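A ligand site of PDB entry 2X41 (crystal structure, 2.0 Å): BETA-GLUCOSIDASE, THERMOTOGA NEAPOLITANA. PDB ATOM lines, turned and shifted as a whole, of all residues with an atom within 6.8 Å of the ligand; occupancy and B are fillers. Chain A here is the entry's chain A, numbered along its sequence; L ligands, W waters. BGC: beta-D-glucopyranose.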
ATOM      1  N   LEU A  25     -14.992  12.265   5.024  1.00  0.00           N
ATOM      2  CA  LEU A  25     -15.715  11.965   3.793  1.00  0.00           C
ATOM      3  C   LEU A  25     -15.303  12.952   2.709  1.00  0.00           C
ATOM      4  O   LEU A  25     -15.529  14.159   2.846  1.00  0.00           O
ATOM      5  CB  LEU A  25     -17.227  12.000   4.002  1.00  0.00           C
ATOM      6  CG  LEU A  25     -18.055  11.342   2.895  1.00  0.00           C
ATOM      7  CD1 LEU A  25     -17.569   9.937   2.611  1.00  0.00           C
ATOM      8  CD2 LEU A  25     -19.533  11.320   3.238  1.00  0.00           C
ATOM      9  N   ALA A  40     -15.191   6.921  -1.926  1.00  0.00           N
ATOM     10  CA  ALA A  40     -15.849   6.868  -0.629  1.00  0.00           C
ATOM     11  C   ALA A  40     -14.946   7.301   0.522  1.00  0.00           C
ATOM     12  O   ALA A  40     -15.425   7.834   1.520  1.00  0.00           O
ATOM     13  CB  ALA A  40     -16.390   5.474  -0.369  1.00  0.00           C
ATOM     14  N   GLY A  41     -13.646   7.079   0.394  1.00  0.00           N
ATOM     15  CA  GLY A  41     -12.719   7.452   1.450  1.00  0.00           C
ATOM     16  C   GLY A  41     -11.264   7.398   1.040  1.00  0.00           C
ATOM     17  O   GLY A  41     -10.907   6.816   0.011  1.00  0.00           O
ATOM     18  N   ALA A  57     -13.306   2.942  -2.720  1.00  0.00           N
ATOM     19  CA  ALA A  57     -14.507   3.340  -3.450  1.00  0.00           C
ATOM     20  C   ALA A  57     -15.547   2.224  -3.575  1.00  0.00           C
ATOM     21  O   ALA A  57     -15.194   1.047  -3.643  1.00  0.00           O
ATOM     22  CB  ALA A  57     -14.131   3.876  -4.844  1.00  0.00           C
ATOM     23  N   ASP A  58     -16.816   2.608  -3.606  1.00  0.00           N
ATOM     24  CA  ASP A  58     -17.901   1.677  -3.912  1.00  0.00           C
ATOM     25  C   ASP A  58     -17.880   1.375  -5.414  1.00  0.00           C
ATOM     26  O   ASP A  58     -17.223   2.082  -6.176  1.00  0.00           O
ATOM     27  CB  ASP A  58     -19.248   2.297  -3.529  1.00  0.00           C
ATOM     28  CG  ASP A  58     -19.389   2.470  -2.027  1.00  0.00           C
ATOM     29  OD1 ASP A  58     -19.545   3.625  -1.567  1.00  0.00           O
ATOM     30  OD2 ASP A  58     -19.324   1.458  -1.309  1.00  0.00           O
ATOM     31  N   GLY A  59     -18.588   0.331  -5.848  1.00  0.00           N
ATOM     32  CA  GLY A  59     -19.362  -0.528  -4.980  1.00  0.00           C
ATOM     33  C   GLY A  59     -19.741  -1.836  -5.674  1.00  0.00           C
ATOM     34  O   GLY A  59     -19.115  -2.203  -6.676  1.00  0.00           O
ATOM     35  N   PRO A  60     -20.750  -2.537  -5.153  1.00  0.00           N
ATOM     36  CA  PRO A  60     -21.157  -3.880  -5.596  1.00  0.00           C
ATOM     37  C   PRO A  60     -21.678  -3.973  -7.044  1.00  0.00           C
ATOM     38  O   PRO A  60     -21.544  -5.043  -7.641  1.00  0.00           O
ATOM     39  CB  PRO A  60     -22.276  -4.253  -4.616  1.00  0.00           C
ATOM     40  CG  PRO A  60     -21.991  -3.429  -3.399  1.00  0.00           C
ATOM     41  CD  PRO A  60     -21.465  -2.122  -3.932  1.00  0.00           C
ATOM     42  N   ARG A  64     -18.185   3.198  -8.266  1.00  0.00           N
ATOM     43  CA  ARG A  64     -18.924   4.447  -8.162  1.00  0.00           C
ATOM     44  C   ARG A  64     -17.986   5.632  -7.906  1.00  0.00           C
ATOM     45  O   ARG A  64     -17.492   5.834  -6.799  1.00  0.00           O
ATOM     46  CB  ARG A  64     -19.982   4.371  -7.066  1.00  0.00           C
ATOM     47  CG  ARG A  64     -20.893   5.584  -6.999  1.00  0.00           C
ATOM     48  CD  ARG A  64     -21.974   5.444  -5.923  1.00  0.00           C
ATOM     49  NE  ARG A  64     -21.382   5.213  -4.605  1.00  0.00           N
ATOM     50  CZ  ARG A  64     -20.882   6.163  -3.835  1.00  0.00           C
ATOM     51  NH1 ARG A  64     -20.872   7.428  -4.243  1.00  0.00           N
ATOM     52  NH2 ARG A  64     -20.368   5.862  -2.653  1.00  0.00           N
ATOM     53  N   LEU A 116     -15.059  -1.399  -2.549  1.00  0.00           N
ATOM     54  CA  LEU A 116     -15.941  -1.711  -1.419  1.00  0.00           C
ATOM     55  C   LEU A 116     -17.015  -2.718  -1.829  1.00  0.00           C
ATOM     56  O   LEU A 116     -18.199  -2.389  -1.893  1.00  0.00           O
ATOM     57  CB  LEU A 116     -16.567  -0.437  -0.854  1.00  0.00           C
ATOM     58  CG  LEU A 116     -15.541   0.613  -0.400  1.00  0.00           C
ATOM     59  CD1 LEU A 116     -16.245   1.834   0.161  1.00  0.00           C
ATOM     60  CD2 LEU A 116     -14.569   0.030   0.624  1.00  0.00           C
ATOM     61  N   ALA A 117     -16.583  -3.945  -2.099  1.00  0.00           N
ATOM     62  CA  ALA A 117     -17.442  -4.988  -2.626  1.00  0.00           C
ATOM     63  C   ALA A 117     -16.698  -6.313  -2.521  1.00  0.00           C
ATOM     64  O   ALA A 117     -15.471  -6.323  -2.481  1.00  0.00           O
ATOM     65  CB  ALA A 117     -17.793  -4.689  -4.085  1.00  0.00           C
ATOM     66  N   ALA A 119     -20.891  -7.025  -1.321  1.00  0.00           N
ATOM     67  CA  ALA A 119     -21.777  -7.141  -0.169  1.00  0.00           C
ATOM     68  C   ALA A 119     -22.315  -8.569  -0.157  1.00  0.00           C
ATOM     69  O   ALA A 119     -22.666  -9.110  -1.197  1.00  0.00           O
ATOM     70  CB  ALA A 119     -22.914  -6.156  -0.268  1.00  0.00           C
ATOM     71  N   ARG A 130     -31.637  -3.559   1.047  1.00  0.00           N
ATOM     72  CA  ARG A 130     -30.389  -3.803   0.320  1.00  0.00           C
ATOM     73  C   ARG A 130     -30.286  -5.217  -0.247  1.00  0.00           C
ATOM     74  O   ARG A 130     -29.238  -5.591  -0.777  1.00  0.00           O
ATOM     75  CB  ARG A 130     -29.177  -3.456   1.186  1.00  0.00           C
ATOM     76  CG  ARG A 130     -29.142  -1.996   1.630  1.00  0.00           C
ATOM     77  CD  ARG A 130     -27.876  -1.663   2.399  1.00  0.00           C
ATOM     78  NE  ARG A 130     -26.722  -1.498   1.522  1.00  0.00           N
ATOM     79  CZ  ARG A 130     -25.543  -1.027   1.928  1.00  0.00           C
ATOM     80  NH1 ARG A 130     -25.386  -0.655   3.191  1.00  0.00           N
ATOM     81  NH2 ARG A 130     -24.540  -0.905   1.073  1.00  0.00           N
ATOM     82  N   GLU A 133     -28.545  -5.855  -3.568  1.00  0.00           N
ATOM     83  CA  GLU A 133     -27.084  -5.916  -3.645  1.00  0.00           C
ATOM     84  C   GLU A 133     -26.442  -6.974  -2.739  1.00  0.00           C
ATOM     85  O   GLU A 133     -25.239  -6.905  -2.449  1.00  0.00           O
ATOM     86  CB  GLU A 133     -26.437  -4.537  -3.440  1.00  0.00           C
ATOM     87  CG  GLU A 133     -26.711  -3.860  -2.107  1.00  0.00           C
ATOM     88  CD  GLU A 133     -26.038  -2.495  -2.016  1.00  0.00           C
ATOM     89  OE1 GLU A 133     -26.452  -1.676  -1.160  1.00  0.00           O
ATOM     90  OE2 GLU A 133     -25.097  -2.230  -2.783  1.00  0.00           O
ATOM     91  N   LYS A 163     -18.482  -7.255   2.769  1.00  0.00           N
ATOM     92  CA  LYS A 163     -19.298  -6.510   3.725  1.00  0.00           C
ATOM     93  C   LYS A 163     -20.703  -7.101   3.748  1.00  0.00           C
ATOM     94  O   LYS A 163     -21.070  -7.817   2.816  1.00  0.00           O
ATOM     95  CB  LYS A 163     -19.317  -5.022   3.336  1.00  0.00           C
ATOM     96  CG  LYS A 163     -19.897  -4.737   1.947  1.00  0.00           C
ATOM     97  CD  LYS A 163     -19.780  -3.246   1.596  1.00  0.00           C
ATOM     98  CE  LYS A 163     -20.573  -2.897   0.338  1.00  0.00           C
ATOM     99  NZ  LYS A 163     -20.422  -1.455  -0.018  1.00  0.00           N
ATOM    100  N   HIS A 164     -21.483  -6.844   4.801  1.00  0.00           N
ATOM    101  CA  HIS A 164     -21.045  -6.149   6.011  1.00  0.00           C
ATOM    102  C   HIS A 164     -21.033  -7.137   7.180  1.00  0.00           C
ATOM    103  O   HIS A 164     -22.048  -7.762   7.490  1.00  0.00           O
ATOM    104  CB  HIS A 164     -21.991  -4.994   6.347  1.00  0.00           C
ATOM    105  CG  HIS A 164     -22.344  -4.143   5.158  1.00  0.00           C
ATOM    106  ND1 HIS A 164     -23.302  -4.497   4.248  1.00  0.00           N
ATOM    107  CD2 HIS A 164     -21.861  -2.946   4.755  1.00  0.00           C
ATOM    108  CE1 HIS A 164     -23.400  -3.560   3.317  1.00  0.00           C
ATOM    109  NE2 HIS A 164     -22.530  -2.607   3.609  1.00  0.00           N
ATOM    110  N   ASN A 168     -26.019  -7.765   9.167  1.00  0.00           N
ATOM    111  CA  ASN A 168     -26.623  -6.505   8.767  1.00  0.00           C
ATOM    112  C   ASN A 168     -27.778  -6.804   7.810  1.00  0.00           C
ATOM    113  O   ASN A 168     -27.653  -6.613   6.592  1.00  0.00           O
ATOM    114  CB  ASN A 168     -25.547  -5.616   8.123  1.00  0.00           C
ATOM    115  CG  ASN A 168     -26.076  -4.274   7.646  1.00  0.00           C
ATOM    116  OD1 ASN A 168     -25.496  -3.668   6.748  1.00  0.00           O
ATOM    117  ND2 ASN A 168     -27.157  -3.794   8.255  1.00  0.00           N
ATOM    118  N   GLU A 171     -32.322  -2.502   7.132  1.00  0.00           N
ATOM    119  CA  GLU A 171     -31.848  -1.124   7.077  1.00  0.00           C
ATOM    120  C   GLU A 171     -32.368  -0.281   8.245  1.00  0.00           C
ATOM    121  O   GLU A 171     -31.691   0.641   8.699  1.00  0.00           O
ATOM    122  CB  GLU A 171     -32.229  -0.479   5.752  1.00  0.00           C
ATOM    123  CG  GLU A 171     -31.467  -1.048   4.562  1.00  0.00           C
ATOM    124  CD  GLU A 171     -29.958  -0.908   4.727  1.00  0.00           C
ATOM    125  OE1 GLU A 171     -29.432   0.203   4.487  1.00  0.00           O
ATOM    126  OE2 GLU A 171     -29.305  -1.902   5.104  1.00  0.00           O
ATOM    127  N   ARG A 174     -30.211   0.621  11.392  1.00  0.00           N
ATOM    128  CA  ARG A 174     -29.024  -0.229  11.283  1.00  0.00           C
ATOM    129  C   ARG A 174     -27.862   0.267  12.140  1.00  0.00           C
ATOM    130  O   ARG A 174     -27.074  -0.520  12.636  1.00  0.00           O
ATOM    131  CB  ARG A 174     -28.583  -0.352   9.817  1.00  0.00           C
ATOM    132  CG  ARG A 174     -28.397   0.994   9.123  1.00  0.00           C
ATOM    133  CD  ARG A 174     -27.885   0.835   7.698  1.00  0.00           C
ATOM    134  NE  ARG A 174     -27.739   2.140   7.047  1.00  0.00           N
ATOM    135  CZ  ARG A 174     -27.010   2.364   5.958  1.00  0.00           C
ATOM    136  NH1 ARG A 174     -26.341   1.361   5.401  1.00  0.00           N
ATOM    137  NH2 ARG A 174     -26.940   3.585   5.443  1.00  0.00           N
ATOM    138  N   MET A 207     -15.290  -5.279   5.941  1.00  0.00           N
ATOM    139  CA  MET A 207     -15.927  -4.114   6.539  1.00  0.00           C
ATOM    140  C   MET A 207     -16.878  -4.543   7.655  1.00  0.00           C
ATOM    141  O   MET A 207     -17.784  -5.345   7.432  1.00  0.00           O
ATOM    142  CB  MET A 207     -16.683  -3.294   5.499  1.00  0.00           C
ATOM    143  CG  MET A 207     -17.349  -2.044   6.074  1.00  0.00           C
ATOM    144  SD  MET A 207     -18.416  -1.194   4.879  1.00  0.00           S
ATOM    145  CE  MET A 207     -17.277  -0.984   3.501  1.00  0.00           C
ATOM    146  N   TYR A 210     -22.722  -1.877  10.674  1.00  0.00           N
ATOM    147  CA  TYR A 210     -23.264  -0.799  11.490  1.00  0.00           C
ATOM    148  C   TYR A 210     -23.865  -1.296  12.794  1.00  0.00           C
ATOM    149  O   TYR A 210     -23.746  -0.627  13.829  1.00  0.00           O
ATOM    150  CB  TYR A 210     -24.355  -0.053  10.721  1.00  0.00           C
ATOM    151  CG  TYR A 210     -23.850   1.035   9.807  1.00  0.00           C
ATOM    152  CD1 TYR A 210     -23.124   2.113  10.313  1.00  0.00           C
ATOM    153  CD2 TYR A 210     -24.103   1.000   8.435  1.00  0.00           C
ATOM    154  CE1 TYR A 210     -22.662   3.120   9.485  1.00  0.00           C
ATOM    155  CE2 TYR A 210     -23.636   2.008   7.599  1.00  0.00           C
ATOM    156  CZ  TYR A 210     -22.924   3.052   8.129  1.00  0.00           C
ATOM    157  OH  TYR A 210     -22.468   4.059   7.309  1.00  0.00           O
ATOM    158  N   ASP A 242     -17.702   0.369   8.776  1.00  0.00           N
ATOM    159  CA  ASP A 242     -18.622   1.002   7.858  1.00  0.00           C
ATOM    160  C   ASP A 242     -18.603   2.487   8.200  1.00  0.00           C
ATOM    161  O   ASP A 242     -18.128   2.865   9.283  1.00  0.00           O
ATOM    162  CB  ASP A 242     -20.031   0.409   7.950  1.00  0.00           C
ATOM    163  CG  ASP A 242     -20.821   0.576   6.659  1.00  0.00           C
ATOM    164  OD1 ASP A 242     -20.503   1.520   5.891  1.00  0.00           O
ATOM    165  OD2 ASP A 242     -21.730  -0.228   6.399  1.00  0.00           O
ATOM    166  N   TRP A 243     -19.078   3.320   7.287  1.00  0.00           N
ATOM    167  CA  TRP A 243     -18.908   4.757   7.389  1.00  0.00           C
ATOM    168  C   TRP A 243     -19.614   5.360   8.604  1.00  0.00           C
ATOM    169  O   TRP A 243     -20.847   5.417   8.646  1.00  0.00           O
ATOM    170  CB  TRP A 243     -19.379   5.437   6.093  1.00  0.00           C
ATOM    171  CG  TRP A 243     -18.313   5.557   5.029  1.00  0.00           C
ATOM    172  CD1 TRP A 243     -18.143   6.607   4.165  1.00  0.00           C
ATOM    173  CD2 TRP A 243     -17.280   4.608   4.713  1.00  0.00           C
ATOM    174  NE1 TRP A 243     -17.073   6.365   3.328  1.00  0.00           N
ATOM    175  CE2 TRP A 243     -16.527   5.147   3.647  1.00  0.00           C
ATOM    176  CE3 TRP A 243     -16.911   3.359   5.227  1.00  0.00           C
ATOM    177  CZ2 TRP A 243     -15.420   4.482   3.089  1.00  0.00           C
ATOM    178  CZ3 TRP A 243     -15.825   2.700   4.668  1.00  0.00           C
ATOM    179  CH2 TRP A 243     -15.094   3.262   3.613  1.00  0.00           C
ATOM    180  N   SER A 370     -25.062   3.774  -1.780  1.00  0.00           N
ATOM    181  CA  SER A 370     -23.627   3.674  -2.041  1.00  0.00           C
ATOM    182  C   SER A 370     -23.344   2.653  -3.143  1.00  0.00           C
ATOM    183  O   SER A 370     -22.277   2.666  -3.742  1.00  0.00           O
ATOM    184  CB  SER A 370     -22.862   3.306  -0.766  1.00  0.00           C
ATOM    185  OG  SER A 370     -23.183   2.003  -0.329  1.00  0.00           O
ATOM    186  N   GLY A 371     -24.308   1.777  -3.395  1.00  0.00           N
ATOM    187  CA  GLY A 371     -24.174   0.752  -4.413  1.00  0.00           C
ATOM    188  C   GLY A 371     -24.735   1.142  -5.772  1.00  0.00           C
ATOM    189  O   GLY A 371     -24.964   0.280  -6.616  1.00  0.00           O
ATOM    190  N   GLU A 458     -30.291   1.447  -0.110  1.00  0.00           N
ATOM    191  CA  GLU A 458     -29.694   1.624   1.200  1.00  0.00           C
ATOM    192  C   GLU A 458     -30.509   2.627   2.020  1.00  0.00           C
ATOM    193  O   GLU A 458     -31.012   3.602   1.464  1.00  0.00           O
ATOM    194  CB  GLU A 458     -28.248   2.107   1.042  1.00  0.00           C
ATOM    195  CG  GLU A 458     -27.465   2.180   2.344  1.00  0.00           C
ATOM    196  CD  GLU A 458     -26.076   2.797   2.159  1.00  0.00           C
ATOM    197  OE1 GLU A 458     -25.587   2.818   1.003  1.00  0.00           O
ATOM    198  OE2 GLU A 458     -25.483   3.247   3.167  1.00  0.00           O
HETATM  199  C2  BGC L   1     -22.560   1.605   3.328  1.00  0.00           C
HETATM  200  C3  BGC L   1     -21.384   0.837   2.736  1.00  0.00           C
HETATM  201  C4  BGC L   1     -20.575   1.750   1.821  1.00  0.00           C
HETATM  202  C5  BGC L   1     -20.147   2.984   2.613  1.00  0.00           C
HETATM  203  C6  BGC L   1     -19.230   3.893   1.800  1.00  0.00           C
HETATM  204  C1  BGC L   1     -22.122   2.954   3.908  1.00  0.00           C
HETATM  205  O1  BGC L   1     -23.255   3.717   4.221  1.00  0.00           O
HETATM  206  O2  BGC L   1     -23.162   0.822   4.343  1.00  0.00           O
HETATM  207  O3  BGC L   1     -21.858  -0.279   2.030  1.00  0.00           O
HETATM  208  O4  BGC L   1     -19.427   1.082   1.335  1.00  0.00           O
HETATM  209  O5  BGC L   1     -21.321   3.670   2.990  1.00  0.00           O
HETATM  210  O6  BGC L   1     -19.987   4.574   0.822  1.00  0.00           O
HETATM  211  O   HOH W   1     -24.040   5.607   1.783  1.00  0.00           O
HETATM  212  O   HOH W   2     -21.766   6.777   1.074  1.00  0.00           O
HETATM  213  O   HOH W   3     -22.751  -0.681  -1.304  1.00  0.00           O
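NH1 of Arg 174 sits at hydrogen-bond distance from O2 of the ligand.
O3 of the ligand sits at hydrogen-bond distance from NZ of Lys 163 (2.8 Å).
NE2 of His 164 is in hydrogen-bond range of O3 of the ligand, at 2.9 Å.
OD2 of Asp 242 sits at hydrogen-bond distance from O2 of the ligand, at 2.7 Å.
An oxygen (O2) of the ligand lies within hydrogen-bond range of the guanidinium group of Arg 130 (2.9 Å).
OH of Tyr 210 is in hydrogen-bond range of O1 of the ligand, 3.2 Å away.
An oxygen (O1) of the ligand lies within hydrogen-bond range of the side-chain carboxylate (OE2) of Glu 458, 2.5 Å away.
OD1 of Asp 58 lies within hydrogen-bond range of O6 of the ligand (2.6 Å).
OD1 of Asp 58 lies within salt-bridge range of NH2 of Arg 64.
The guanidinium group (NH2) of Arg 130 is in salt-bridge range of the side-chain carboxylate (OE1) of Glu 458.
O of Ala 57 lies within hydrogen-bond range of N of Leu 116 (2.7 Å).
A ring nitrogen (NE2) of His 164 is in hydrogen-bond range of the guanidinium group (NH1) of Arg 130 (3.5 Å).
The side-chain amino group (NZ) of Lys 163 is in salt-bridge range of the side-chain carboxylate (OD2) of Asp 58, at 3.4 Å.
NE1 of Trp 243 lies within hydrogen-bond range of O of Ala 40 (2.9 Å).
The side-chain carboxylate (OE1) of Glu 458 lies within hydrogen-bond range of the side-chain hydroxyl (OG) of Ser 370, 2.9 Å away.
The backbone carbonyl oxygen (O) of Ser 370 is in hydrogen-bond range of the guanidinium group (NE) of Arg 64.
CB of Ala 40 touches O6 of the ligand, at 3.9 Å.
NH2 of Arg 64 touches O6 of the ligand (3.7 Å).
CD1 of Leu 116 touches O4 of the ligand, 3.5 Å away.
CE of Met 207 touches O4 of the ligand (3.7 Å).
CE2 of Trp 243 touches C6 of the ligand, 3.5 Å away.
Ser 370 touches the ligand (OG to C4, 3.4 Å).
Hydrophobic or aromatic side chains within 4 Å of the ligand: Ala 40, Leu 116, His 164, Met 207, Tyr 210 and Trp 243.
Water W1 lies within hydrogen-bond range of OE2 of Glu 458 (3.1 Å) and O1 of the ligand (3.2 Å).
Water W3 lies within hydrogen-bond range of the side-chain amino group of Lys 163 (2.8 Å), the side-chain hydroxyl of Ser 370 (2.9 Å), the guanidinium group of Arg 130 (3.0 Å), the side-chain carboxylate of Glu 133 (3.2 Å) and an oxygen (O3) of the ligand (3.5 Å).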
